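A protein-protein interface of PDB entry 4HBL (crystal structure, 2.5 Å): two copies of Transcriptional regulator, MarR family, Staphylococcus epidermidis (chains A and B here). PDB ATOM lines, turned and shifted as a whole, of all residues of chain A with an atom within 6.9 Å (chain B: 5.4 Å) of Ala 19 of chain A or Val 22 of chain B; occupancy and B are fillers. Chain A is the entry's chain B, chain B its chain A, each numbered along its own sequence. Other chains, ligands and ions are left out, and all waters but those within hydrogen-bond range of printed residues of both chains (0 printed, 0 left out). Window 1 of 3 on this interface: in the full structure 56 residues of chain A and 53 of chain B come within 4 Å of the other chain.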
ATOM      1  N   GLN A  14      22.285  -9.603  15.066  1.00  0.00           N
ATOM      2  CA  GLN A  14      20.946  -9.043  15.195  1.00  0.00           C
ATOM      3  C   GLN A  14      19.958 -10.022  14.603  1.00  0.00           C
ATOM      4  O   GLN A  14      18.834 -10.139  15.075  1.00  0.00           O
ATOM      5  CB  GLN A  14      20.853  -7.701  14.445  1.00  0.00           C
ATOM      6  CG  GLN A  14      19.933  -6.639  15.057  1.00  0.00           C
ATOM      7  CD  GLN A  14      19.973  -5.281  14.321  1.00  0.00           C
ATOM      8  OE1 GLN A  14      18.944  -4.595  14.201  1.00  0.00           O
ATOM      9  NE2 GLN A  14      21.161  -4.887  13.826  1.00  0.00           N
ATOM     10  N   LEU A  15      20.379 -10.731  13.564  1.00  0.00           N
ATOM     11  CA  LEU A  15      19.480 -11.651  12.887  1.00  0.00           C
ATOM     12  C   LEU A  15      19.304 -12.935  13.670  1.00  0.00           C
ATOM     13  O   LEU A  15      18.266 -13.578  13.649  1.00  0.00           O
ATOM     14  CB  LEU A  15      19.997 -11.981  11.497  1.00  0.00           C
ATOM     15  CG  LEU A  15      19.880 -10.827  10.517  1.00  0.00           C
ATOM     16  CD1 LEU A  15      20.475 -11.245   9.175  1.00  0.00           C
ATOM     17  CD2 LEU A  15      18.422 -10.385  10.408  1.00  0.00           C
ATOM     18  N   CYS A  16      20.341 -13.293  14.398  1.00  0.00           N
ATOM     19  CA  CYS A  16      20.268 -14.406  15.282  1.00  0.00           C
ATOM     20  C   CYS A  16      19.298 -14.164  16.450  1.00  0.00           C
ATOM     21  O   CYS A  16      18.563 -15.030  16.827  1.00  0.00           O
ATOM     22  CB  CYS A  16      21.654 -14.695  15.790  1.00  0.00           C
ATOM     23  SG  CYS A  16      21.523 -15.996  17.011  1.00  0.00           S
ATOM     24  N   PHE A  17      19.303 -12.975  17.026  1.00  0.00           N
ATOM     25  CA  PHE A  17      18.365 -12.645  18.076  1.00  0.00           C
ATOM     26  C   PHE A  17      16.963 -12.431  17.521  1.00  0.00           C
ATOM     27  O   PHE A  17      15.977 -12.686  18.235  1.00  0.00           O
ATOM     28  CB  PHE A  17      18.837 -11.417  18.854  1.00  0.00           C
ATOM     29  CG  PHE A  17      19.994 -11.705  19.769  1.00  0.00           C
ATOM     30  CD1 PHE A  17      20.834 -12.814  19.541  1.00  0.00           C
ATOM     31  CD2 PHE A  17      20.255 -10.885  20.861  1.00  0.00           C
ATOM     32  CE1 PHE A  17      21.894 -13.095  20.377  1.00  0.00           C
ATOM     33  CE2 PHE A  17      21.319 -11.163  21.710  1.00  0.00           C
ATOM     34  CZ  PHE A  17      22.136 -12.269  21.465  1.00  0.00           C
ATOM     35  N   SER A  18      16.864 -11.977  16.272  1.00  0.00           N
ATOM     36  CA  SER A  18      15.551 -11.706  15.668  1.00  0.00           C
ATOM     37  C   SER A  18      14.899 -13.009  15.279  1.00  0.00           C
ATOM     38  O   SER A  18      13.689 -13.153  15.368  1.00  0.00           O
ATOM     39  CB  SER A  18      15.677 -10.812  14.430  1.00  0.00           C
ATOM     40  OG  SER A  18      16.049  -9.446  14.755  1.00  0.00           O
ATOM     41  N   ALA A  19      15.707 -13.975  14.861  1.00  0.00           N
ATOM     42  CA  ALA A  19      15.175 -15.241  14.448  1.00  0.00           C
ATOM     43  C   ALA A  19      14.645 -15.945  15.695  1.00  0.00           C
ATOM     44  O   ALA A  19      13.597 -16.581  15.678  1.00  0.00           O
ATOM     45  CB  ALA A  19      16.269 -16.065  13.759  1.00  0.00           C
ATOM     46  N   TYR A  20      15.369 -15.820  16.786  1.00  0.00           N
ATOM     47  CA  TYR A  20      14.878 -16.347  18.053  1.00  0.00           C
ATOM     48  C   TYR A  20      13.560 -15.678  18.513  1.00  0.00           C
ATOM     49  O   TYR A  20      12.647 -16.336  19.006  1.00  0.00           O
ATOM     50  CB  TYR A  20      15.950 -16.253  19.144  1.00  0.00           C
ATOM     51  CG  TYR A  20      15.337 -16.374  20.546  1.00  0.00           C
ATOM     52  CD1 TYR A  20      15.118 -15.232  21.366  1.00  0.00           C
ATOM     53  CD2 TYR A  20      14.924 -17.628  21.050  1.00  0.00           C
ATOM     54  CE1 TYR A  20      14.538 -15.353  22.626  1.00  0.00           C
ATOM     55  CE2 TYR A  20      14.342 -17.747  22.309  1.00  0.00           C
ATOM     56  CZ  TYR A  20      14.153 -16.621  23.092  1.00  0.00           C
ATOM     57  OH  TYR A  20      13.574 -16.789  24.337  1.00  0.00           O
ATOM     58  N   ASN A  21      13.469 -14.377  18.328  1.00  0.00           N
ATOM     59  CA  ASN A  21      12.324 -13.608  18.715  1.00  0.00           C
ATOM     60  C   ASN A  21      11.098 -14.030  17.955  1.00  0.00           C
ATOM     61  O   ASN A  21      10.038 -14.242  18.569  1.00  0.00           O
ATOM     62  CB  ASN A  21      12.602 -12.136  18.451  1.00  0.00           C
ATOM     63  CG  ASN A  21      12.057 -11.234  19.522  1.00  0.00           C
ATOM     64  OD1 ASN A  21      11.181 -11.621  20.313  1.00  0.00           O
ATOM     65  ND2 ASN A  21      12.577 -10.011  19.566  1.00  0.00           N
ATOM     66  N   VAL A  22      11.245 -14.140  16.629  1.00  0.00           N
ATOM     67  CA  VAL A  22      10.151 -14.491  15.699  1.00  0.00           C
ATOM     68  C   VAL A  22       9.638 -15.895  16.043  1.00  0.00           C
ATOM     69  O   VAL A  22       8.448 -16.141  16.174  1.00  0.00           O
ATOM     70  CB  VAL A  22      10.652 -14.453  14.249  1.00  0.00           C
ATOM     71  CG1 VAL A  22       9.872 -15.383  13.321  1.00  0.00           C
ATOM     72  CG2 VAL A  22      10.591 -13.049  13.722  1.00  0.00           C
ATOM     73  N   SER A  23      10.555 -16.815  16.251  1.00  0.00           N
ATOM     74  CA  SER A  23      10.153 -18.148  16.568  1.00  0.00           C
ATOM     75  C   SER A  23       9.365 -18.128  17.906  1.00  0.00           C
ATOM     76  O   SER A  23       8.299 -18.745  18.008  1.00  0.00           O
ATOM     77  CB  SER A  23      11.392 -19.044  16.559  1.00  0.00           C
ATOM     78  OG  SER A  23      11.001 -20.361  16.790  1.00  0.00           O
ATOM     79  N   ARG A  24       9.835 -17.378  18.898  1.00  0.00           N
ATOM     80  CA  ARG A  24       9.143 -17.317  20.184  1.00  0.00           C
ATOM     81  C   ARG A  24       7.760 -16.744  20.044  1.00  0.00           C
ATOM     82  O   ARG A  24       6.830 -17.175  20.733  1.00  0.00           O
ATOM     83  CB  ARG A  24       9.914 -16.442  21.187  1.00  0.00           C
ATOM     84  CG  ARG A  24       9.372 -16.517  22.620  1.00  0.00           C
ATOM     85  CD  ARG A  24      10.058 -15.562  23.602  1.00  0.00           C
ATOM     86  NE  ARG A  24      10.251 -14.224  23.013  1.00  0.00           N
ATOM     87  CZ  ARG A  24       9.316 -13.267  22.880  1.00  0.00           C
ATOM     88  NH1 ARG A  24       8.063 -13.426  23.321  1.00  0.00           N
ATOM     89  NH2 ARG A  24       9.650 -12.128  22.287  1.00  0.00           N
ATOM     90  N   VAL A 135      13.473 -14.956   2.538  1.00  0.00           N
ATOM     91  CA  VAL A 135      14.514 -14.574   3.485  1.00  0.00           C
ATOM     92  C   VAL A 135      14.795 -15.724   4.438  1.00  0.00           C
ATOM     93  O   VAL A 135      15.949 -16.070   4.609  1.00  0.00           O
ATOM     94  CB  VAL A 135      14.128 -13.278   4.239  1.00  0.00           C
ATOM     95  CG1 VAL A 135      15.006 -13.053   5.484  1.00  0.00           C
ATOM     96  CG2 VAL A 135      14.117 -12.109   3.269  1.00  0.00           C
ATOM     97  N   PHE A 136      13.749 -16.312   5.037  1.00  0.00           N
ATOM     98  CA  PHE A 136      13.892 -17.494   5.893  1.00  0.00           C
ATOM     99  C   PHE A 136      14.452 -18.697   5.181  1.00  0.00           C
ATOM    100  O   PHE A 136      15.203 -19.454   5.780  1.00  0.00           O
ATOM    101  CB  PHE A 136      12.594 -17.853   6.572  1.00  0.00           C
ATOM    102  CG  PHE A 136      12.300 -16.987   7.766  1.00  0.00           C
ATOM    103  CD1 PHE A 136      12.823 -17.300   9.008  1.00  0.00           C
ATOM    104  CD2 PHE A 136      11.539 -15.831   7.633  1.00  0.00           C
ATOM    105  CE1 PHE A 136      12.584 -16.495  10.102  1.00  0.00           C
ATOM    106  CE2 PHE A 136      11.285 -15.025   8.733  1.00  0.00           C
ATOM    107  CZ  PHE A 136      11.818 -15.360   9.956  1.00  0.00           C
ATOM    108  N   GLU A 137      14.090 -18.862   3.909  1.00  0.00           N
ATOM    109  CA  GLU A 137      14.559 -19.981   3.122  1.00  0.00           C
ATOM    110  C   GLU A 137      16.048 -19.797   2.808  1.00  0.00           C
ATOM    111  O   GLU A 137      16.829 -20.734   2.952  1.00  0.00           O
ATOM    112  CB  GLU A 137      13.681 -20.189   1.876  1.00  0.00           C
ATOM    113  CG  GLU A 137      14.040 -21.388   0.991  1.00  0.00           C
ATOM    114  CD  GLU A 137      13.925 -22.746   1.704  1.00  0.00           C
ATOM    115  OE1 GLU A 137      14.983 -23.421   1.935  1.00  0.00           O
ATOM    116  OE2 GLU A 137      12.771 -23.136   2.037  1.00  0.00           O
ATOM    117  N   GLU A 138      16.455 -18.584   2.449  1.00  0.00           N
ATOM    118  CA  GLU A 138      17.878 -18.325   2.186  1.00  0.00           C
ATOM    119  C   GLU A 138      18.769 -18.448   3.409  1.00  0.00           C
ATOM    120  O   GLU A 138      19.904 -18.941   3.316  1.00  0.00           O
ATOM    121  CB  GLU A 138      18.070 -16.951   1.577  1.00  0.00           C
ATOM    122  CG  GLU A 138      17.475 -16.783   0.200  1.00  0.00           C
ATOM    123  CD  GLU A 138      18.169 -17.629  -0.830  1.00  0.00           C
ATOM    124  OE1 GLU A 138      17.941 -18.857  -0.817  1.00  0.00           O
ATOM    125  OE2 GLU A 138      18.931 -17.069  -1.652  1.00  0.00           O
ATOM    126  N   LEU A 139      18.268 -17.995   4.562  1.00  0.00           N
ATOM    127  CA  LEU A 139      18.999 -18.195   5.825  1.00  0.00           C
ATOM    128  C   LEU A 139      19.091 -19.671   6.227  1.00  0.00           C
ATOM    129  O   LEU A 139      20.146 -20.127   6.616  1.00  0.00           O
ATOM    130  CB  LEU A 139      18.392 -17.383   6.987  1.00  0.00           C
ATOM    131  CG  LEU A 139      18.817 -15.955   7.348  1.00  0.00           C
ATOM    132  CD1 LEU A 139      20.330 -15.864   7.577  1.00  0.00           C
ATOM    133  CD2 LEU A 139      18.431 -15.019   6.238  1.00  0.00           C
ATOM    134  N   GLU A 140      17.975 -20.398   6.165  1.00  0.00           N
ATOM    135  CA  GLU A 140      17.976 -21.812   6.489  1.00  0.00           C
ATOM    136  C   GLU A 140      18.961 -22.562   5.571  1.00  0.00           C
ATOM    137  O   GLU A 140      19.808 -23.341   6.033  1.00  0.00           O
ATOM    138  CB  GLU A 140      16.584 -22.365   6.299  1.00  0.00           C
ATOM    139  CG  GLU A 140      16.381 -23.750   6.887  1.00  0.00           C
ATOM    140  CD  GLU A 140      14.941 -24.245   6.789  1.00  0.00           C
ATOM    141  OE1 GLU A 140      14.002 -23.444   6.447  1.00  0.00           O
ATOM    142  OE2 GLU A 140      14.746 -25.456   7.067  1.00  0.00           O
ATOM    143  N   GLN A 141      18.869 -22.290   4.271  1.00  0.00           N
ATOM    144  CA  GLN A 141      19.685 -22.966   3.300  1.00  0.00           C
ATOM    145  C   GLN A 141      21.183 -22.779   3.604  1.00  0.00           C
ATOM    146  O   GLN A 141      21.910 -23.735   3.560  1.00  0.00           O
ATOM    147  CB  GLN A 141      19.272 -22.546   1.874  1.00  0.00           C
ATOM    148  CG  GLN A 141      19.932 -23.292   0.719  1.00  0.00           C
ATOM    149  CD  GLN A 141      19.686 -24.798   0.754  1.00  0.00           C
ATOM    150  OE1 GLN A 141      18.541 -25.244   0.857  1.00  0.00           O
ATOM    151  NE2 GLN A 141      20.762 -25.590   0.663  1.00  0.00           N
ATOM    152  N   LEU A 143      22.634 -21.898   6.576  1.00  0.00           N
ATOM    153  CA  LEU A 143      22.955 -22.579   7.827  1.00  0.00           C
ATOM    154  C   LEU A 143      23.185 -24.107   7.667  1.00  0.00           C
ATOM    155  O   LEU A 143      24.231 -24.649   8.096  1.00  0.00           O
ATOM    156  CB  LEU A 143      21.942 -22.195   8.910  1.00  0.00           C
ATOM    157  CG  LEU A 143      21.978 -20.700   9.349  1.00  0.00           C
ATOM    158  CD1 LEU A 143      20.672 -20.202   9.895  1.00  0.00           C
ATOM    159  CD2 LEU A 143      23.047 -20.397  10.384  1.00  0.00           C
ATOM    160  N   SER B  18       9.678 -22.859   9.147  1.00  0.00           N
ATOM    161  CA  SER B  18      10.986 -22.406   8.706  1.00  0.00           C
ATOM    162  C   SER B  18      11.712 -21.608   9.818  1.00  0.00           C
ATOM    163  O   SER B  18      12.917 -21.776  10.019  1.00  0.00           O
ATOM    164  CB  SER B  18      10.813 -21.581   7.437  1.00  0.00           C
ATOM    165  OG  SER B  18      12.060 -21.280   6.856  1.00  0.00           O
ATOM    166  N   ALA B  19      10.961 -20.759  10.531  1.00  0.00           N
ATOM    167  CA  ALA B  19      11.490 -19.844  11.543  1.00  0.00           C
ATOM    168  C   ALA B  19      12.024 -20.609  12.686  1.00  0.00           C
ATOM    169  O   ALA B  19      12.967 -20.178  13.323  1.00  0.00           O
ATOM    170  CB  ALA B  19      10.403 -18.910  12.061  1.00  0.00           C
ATOM    171  N   TYR B  20      11.369 -21.723  12.971  1.00  0.00           N
ATOM    172  CA  TYR B  20      11.766 -22.603  14.038  1.00  0.00           C
ATOM    173  C   TYR B  20      13.065 -23.251  13.695  1.00  0.00           C
ATOM    174  O   TYR B  20      13.935 -23.416  14.558  1.00  0.00           O
ATOM    175  CB  TYR B  20      10.718 -23.695  14.253  1.00  0.00           C
ATOM    176  CG  TYR B  20      10.971 -24.615  15.430  1.00  0.00           C
ATOM    177  CD1 TYR B  20      11.445 -25.902  15.235  1.00  0.00           C
ATOM    178  CD2 TYR B  20      10.727 -24.189  16.721  1.00  0.00           C
ATOM    179  CE1 TYR B  20      11.652 -26.751  16.291  1.00  0.00           C
ATOM    180  CE2 TYR B  20      10.923 -25.019  17.802  1.00  0.00           C
ATOM    181  CZ  TYR B  20      11.374 -26.296  17.576  1.00  0.00           C
ATOM    182  OH  TYR B  20      11.567 -27.101  18.635  1.00  0.00           O
ATOM    183  N   ASN B  21      13.225 -23.614  12.437  1.00  0.00           N
ATOM    184  CA  ASN B  21      14.488 -24.214  11.980  1.00  0.00           C
ATOM    185  C   ASN B  21      15.632 -23.235  12.042  1.00  0.00           C
ATOM    186  O   ASN B  21      16.658 -23.516  12.635  1.00  0.00           O
ATOM    187  CB  ASN B  21      14.330 -24.825  10.589  1.00  0.00           C
ATOM    188  CG  ASN B  21      13.651 -26.180  10.640  1.00  0.00           C
ATOM    189  OD1 ASN B  21      14.254 -27.157  11.068  1.00  0.00           O
ATOM    190  ND2 ASN B  21      12.395 -26.249  10.211  1.00  0.00           N
ATOM    191  N   VAL B  22      15.415 -22.061  11.453  1.00  0.00           N
ATOM    192  CA  VAL B  22      16.387 -20.981  11.426  1.00  0.00           C
ATOM    193  C   VAL B  22      16.847 -20.615  12.830  1.00  0.00           C
ATOM    194  O   VAL B  22      18.045 -20.549  13.077  1.00  0.00           O
ATOM    195  CB  VAL B  22      15.797 -19.762  10.714  1.00  0.00           C
ATOM    196  CG1 VAL B  22      16.680 -18.551  10.898  1.00  0.00           C
ATOM    197  CG2 VAL B  22      15.664 -20.089   9.244  1.00  0.00           C
ATOM    198  N   SER B  23      15.916 -20.436  13.764  1.00  0.00           N
ATOM    199  CA  SER B  23      16.331 -20.068  15.123  1.00  0.00           C
ATOM    200  C   SER B  23      17.192 -21.132  15.775  1.00  0.00           C
ATOM    201  O   SER B  23      18.136 -20.812  16.468  1.00  0.00           O
ATOM    202  CB  SER B  23      15.163 -19.714  16.010  1.00  0.00           C
ATOM    203  OG  SER B  23      14.397 -20.860  16.243  1.00  0.00           O
ATOM    204  N   ARG B  24      16.923 -22.401  15.520  1.00  0.00           N
ATOM    205  CA  ARG B  24      17.723 -23.448  16.155  1.00  0.00           C
ATOM    206  C   ARG B  24      19.048 -23.624  15.465  1.00  0.00           C
ATOM    207  O   ARG B  24      20.040 -23.981  16.126  1.00  0.00           O
ATOM    208  CB  ARG B  24      16.992 -24.779  16.129  1.00  0.00           C
ATOM    209  CG  ARG B  24      15.770 -24.813  17.000  1.00  0.00           C
ATOM    210  CD  ARG B  24      15.187 -26.215  16.920  1.00  0.00           C
ATOM    211  NE  ARG B  24      16.189 -27.221  17.267  1.00  0.00           N
ATOM    212  CZ  ARG B  24      16.559 -27.485  18.515  1.00  0.00           C
ATOM    213  NH1 ARG B  24      16.005 -26.800  19.520  1.00  0.00           N
ATOM    214  NH2 ARG B  24      17.473 -28.428  18.758  1.00  0.00           N
ATOM    215  N   LEU B  25      19.079 -23.377  14.152  1.00  0.00           N
ATOM    216  CA  LEU B  25      20.307 -23.549  13.414  1.00  0.00           C
ATOM    217  C   LEU B  25      21.251 -22.425  13.727  1.00  0.00           C
ATOM    218  O   LEU B  25      22.466 -22.611  13.817  1.00  0.00           O
ATOM    219  CB  LEU B  25      20.063 -23.661  11.916  1.00  0.00           C
ATOM    220  CG  LEU B  25      19.490 -24.980  11.409  1.00  0.00           C
ATOM    221  CD1 LEU B  25      18.749 -24.748  10.080  1.00  0.00           C
ATOM    222  CD2 LEU B  25      20.520 -26.085  11.272  1.00  0.00           C
ATOM    223  N   PHE B  26      20.708 -21.248  13.881  1.00  0.00           N
ATOM    224  CA  PHE B  26      21.522 -20.099  14.331  1.00  0.00           C
ATOM    225  C   PHE B  26      22.239 -20.315  15.665  1.00  0.00           C
ATOM    226  O   PHE B  26      23.413 -19.995  15.791  1.00  0.00           O
ATOM    227  CB  PHE B  26      20.670 -18.843  14.454  1.00  0.00           C
ATOM    228  CG  PHE B  26      20.848 -17.841  13.347  1.00  0.00           C
ATOM    229  CD1 PHE B  26      22.094 -17.341  13.026  1.00  0.00           C
ATOM    230  CD2 PHE B  26      19.715 -17.289  12.708  1.00  0.00           C
ATOM    231  CE1 PHE B  26      22.227 -16.364  12.060  1.00  0.00           C
ATOM    232  CE2 PHE B  26      19.846 -16.317  11.732  1.00  0.00           C
ATOM    233  CZ  PHE B  26      21.103 -15.852  11.416  1.00  0.00           C
ATOM    234  N   ALA B  27      21.528 -20.823  16.659  1.00  0.00           N
ATOM    235  CA  ALA B  27      22.130 -21.143  17.990  1.00  0.00           C
ATOM    236  C   ALA B  27      23.180 -22.244  17.836  1.00  0.00           C
ATOM    237  O   ALA B  27      24.219 -22.249  18.517  1.00  0.00           O
ATOM    238  CB  ALA B  27      21.046 -21.554  19.005  1.00  0.00           C
ATOM    239  N   PHE B 136      12.237  -8.987   8.961  1.00  0.00           N
ATOM    240  CA  PHE B 136      12.183  -9.422  10.355  1.00  0.00           C
ATOM    241  C   PHE B 136      11.382  -8.487  11.241  1.00  0.00           C
ATOM    242  O   PHE B 136      10.532  -8.958  11.967  1.00  0.00           O
ATOM    243  CB  PHE B 136      13.581  -9.629  10.924  1.00  0.00           C
ATOM    244  CG  PHE B 136      14.106 -11.000  10.675  1.00  0.00           C
ATOM    245  CD1 PHE B 136      13.813 -12.033  11.531  1.00  0.00           C
ATOM    246  CD2 PHE B 136      14.842 -11.271   9.564  1.00  0.00           C
ATOM    247  CE1 PHE B 136      14.271 -13.315  11.278  1.00  0.00           C
ATOM    248  CE2 PHE B 136      15.309 -12.559   9.306  1.00  0.00           C
ATOM    249  CZ  PHE B 136      15.022 -13.574  10.155  1.00  0.00           C
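Ser 18 of chain A touches Phe 136 of chain B, and with the chains exchanged Phe 136 of chain A touches Ser 18 of chain B. Ala 19 of chain A touches Val 22 of chain B, and with the chains exchanged Val 22 of chain A touches Ala 19 of chain B. Ala 19 of chain A touches Ser 23 of chain B, and with the chains exchanged Ser 23 of chain A touches Ala 19 of chain B. Ala 19 of chain A touches Phe 136 of chain B, and with the chains exchanged Phe 136 of chain A touches Ala 19 of chain B. Positions printed for both chains: 18, 19, 20, 21, 22, 23, 24 and 136. Of the 23 pairs that touch across the chains among the printed residues, 12 have their exchanged pair printed and touching as well.
Hydrophobic or aromatic side chains of chain A within 4 Å of the printed part of chain B: Leu 15, Ala 19, Val 22, Val 135, Phe 136, Leu 139 and Leu 143. Of the 11 printed residues of chain B, 9 touch a printed residue of chain A. Printed residues of chain B that touch a printed residue of chain A: Ser 18, Ala 19, Tyr 20, Asn 21, Val 22, Ser 23, Leu 25, Phe 26 and Phe 136. Hydrophobic or aromatic side chains of chain B that line the printed part of chain A: Ala 19, Tyr 20, Val 22, Leu 25, Phe 26 and Phe 136. Among the printed residues, 23 pairs touch across the chains. Among the printed residues, no Asp or Glu carboxylate lies within 4 Å of a Lys or Arg side-chain nitrogen of the other chain.
CE2 of Phe 26 of chain B touches O of Leu 15 of chain A, 3.7 Å away. Leu 15 of chain A touches Phe 136 of chain B (CD2 to CD2, 3.8 Å). Cys 16 of chain A touches Phe 26 of chain B (CB to CD1, 3.9 Å). Ala 19 of chain A touches Val 22 of chain B (CB to CG1, 3.8 Å). Ala 19 of chain A touches Ser 23 of chain B (O to CB, 3.5 Å). CB of Ala 19 of chain A touches CD2 of Phe 26 of chain B (3.8 Å). Phe 136 of chain B touches Ala 19 of chain A (CE1 to CA, 3.8 Å). Phe 136 of chain A touches Val 22 of chain B (O to CG2, 3.6 Å). OE2 of Glu 140 of chain A touches CB of Asn 21 of chain B (3.6 Å). CB of Glu 140 of chain A touches CG2 of Val 22 of chain B, 3.8 Å away.
Ala 19 of chain A touches just these residues of chain B: Val 22 (3.8 Å), Ser 23 (3.5 Å), Phe 26 (3.8 Å) and Phe 136 (3.8 Å). Val 22 of chain B touches just these residues of chain A: Ala 19, Phe 136 and Glu 140. Printed residues of chain A within 4 Å of Ser 23 of chain B: Ala 19 (3.5 Å), Tyr 20 (3.9 Å) and Ser 23 (3.5 Å). Of the printed residues of chain B, Val 22 of chain A touches Ala 19. Printed residues of chain A within 4 Å of Asn 21 of chain B: Glu 140. Printed residues of chain A within 4 Å of Phe 26 of chain B: Leu 15 (3.7 Å), Cys 16 (3.9 Å), Ala 19 (3.8 Å) and Leu 139 (3.9 Å). Phe 17 of chain A touches none of the printed residues of chain B. The nearest residue of chain B that does not touch Ala 19 of chain A is Ala 19 of chain B (4.3 Å). The nearest printed residue of chain A that does not touch Tyr 20 of chain B is Phe 136 of chain A (6.1 Å).
OE1 of Glu 140 of chain A sits at hydrogen-bond distance from OG of Ser 18 of chain B. OG of Ser 23 of chain B sits at hydrogen-bond distance from OG of Ser 23 of chain A, 3.5 Å away.
OG of Ser 23 of chain B lies within hydrogen-bond range of O of Ala 19 of chain B (3.3 Å). OG of Ser 23 of chain B is in hydrogen-bond range of O of Tyr 20 of chain B. The backbone carbonyl oxygen of Gln 14 of chain A lies within hydrogen-bond range of the side-chain hydroxyl of Ser 18 of chain A (2.9 Å).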
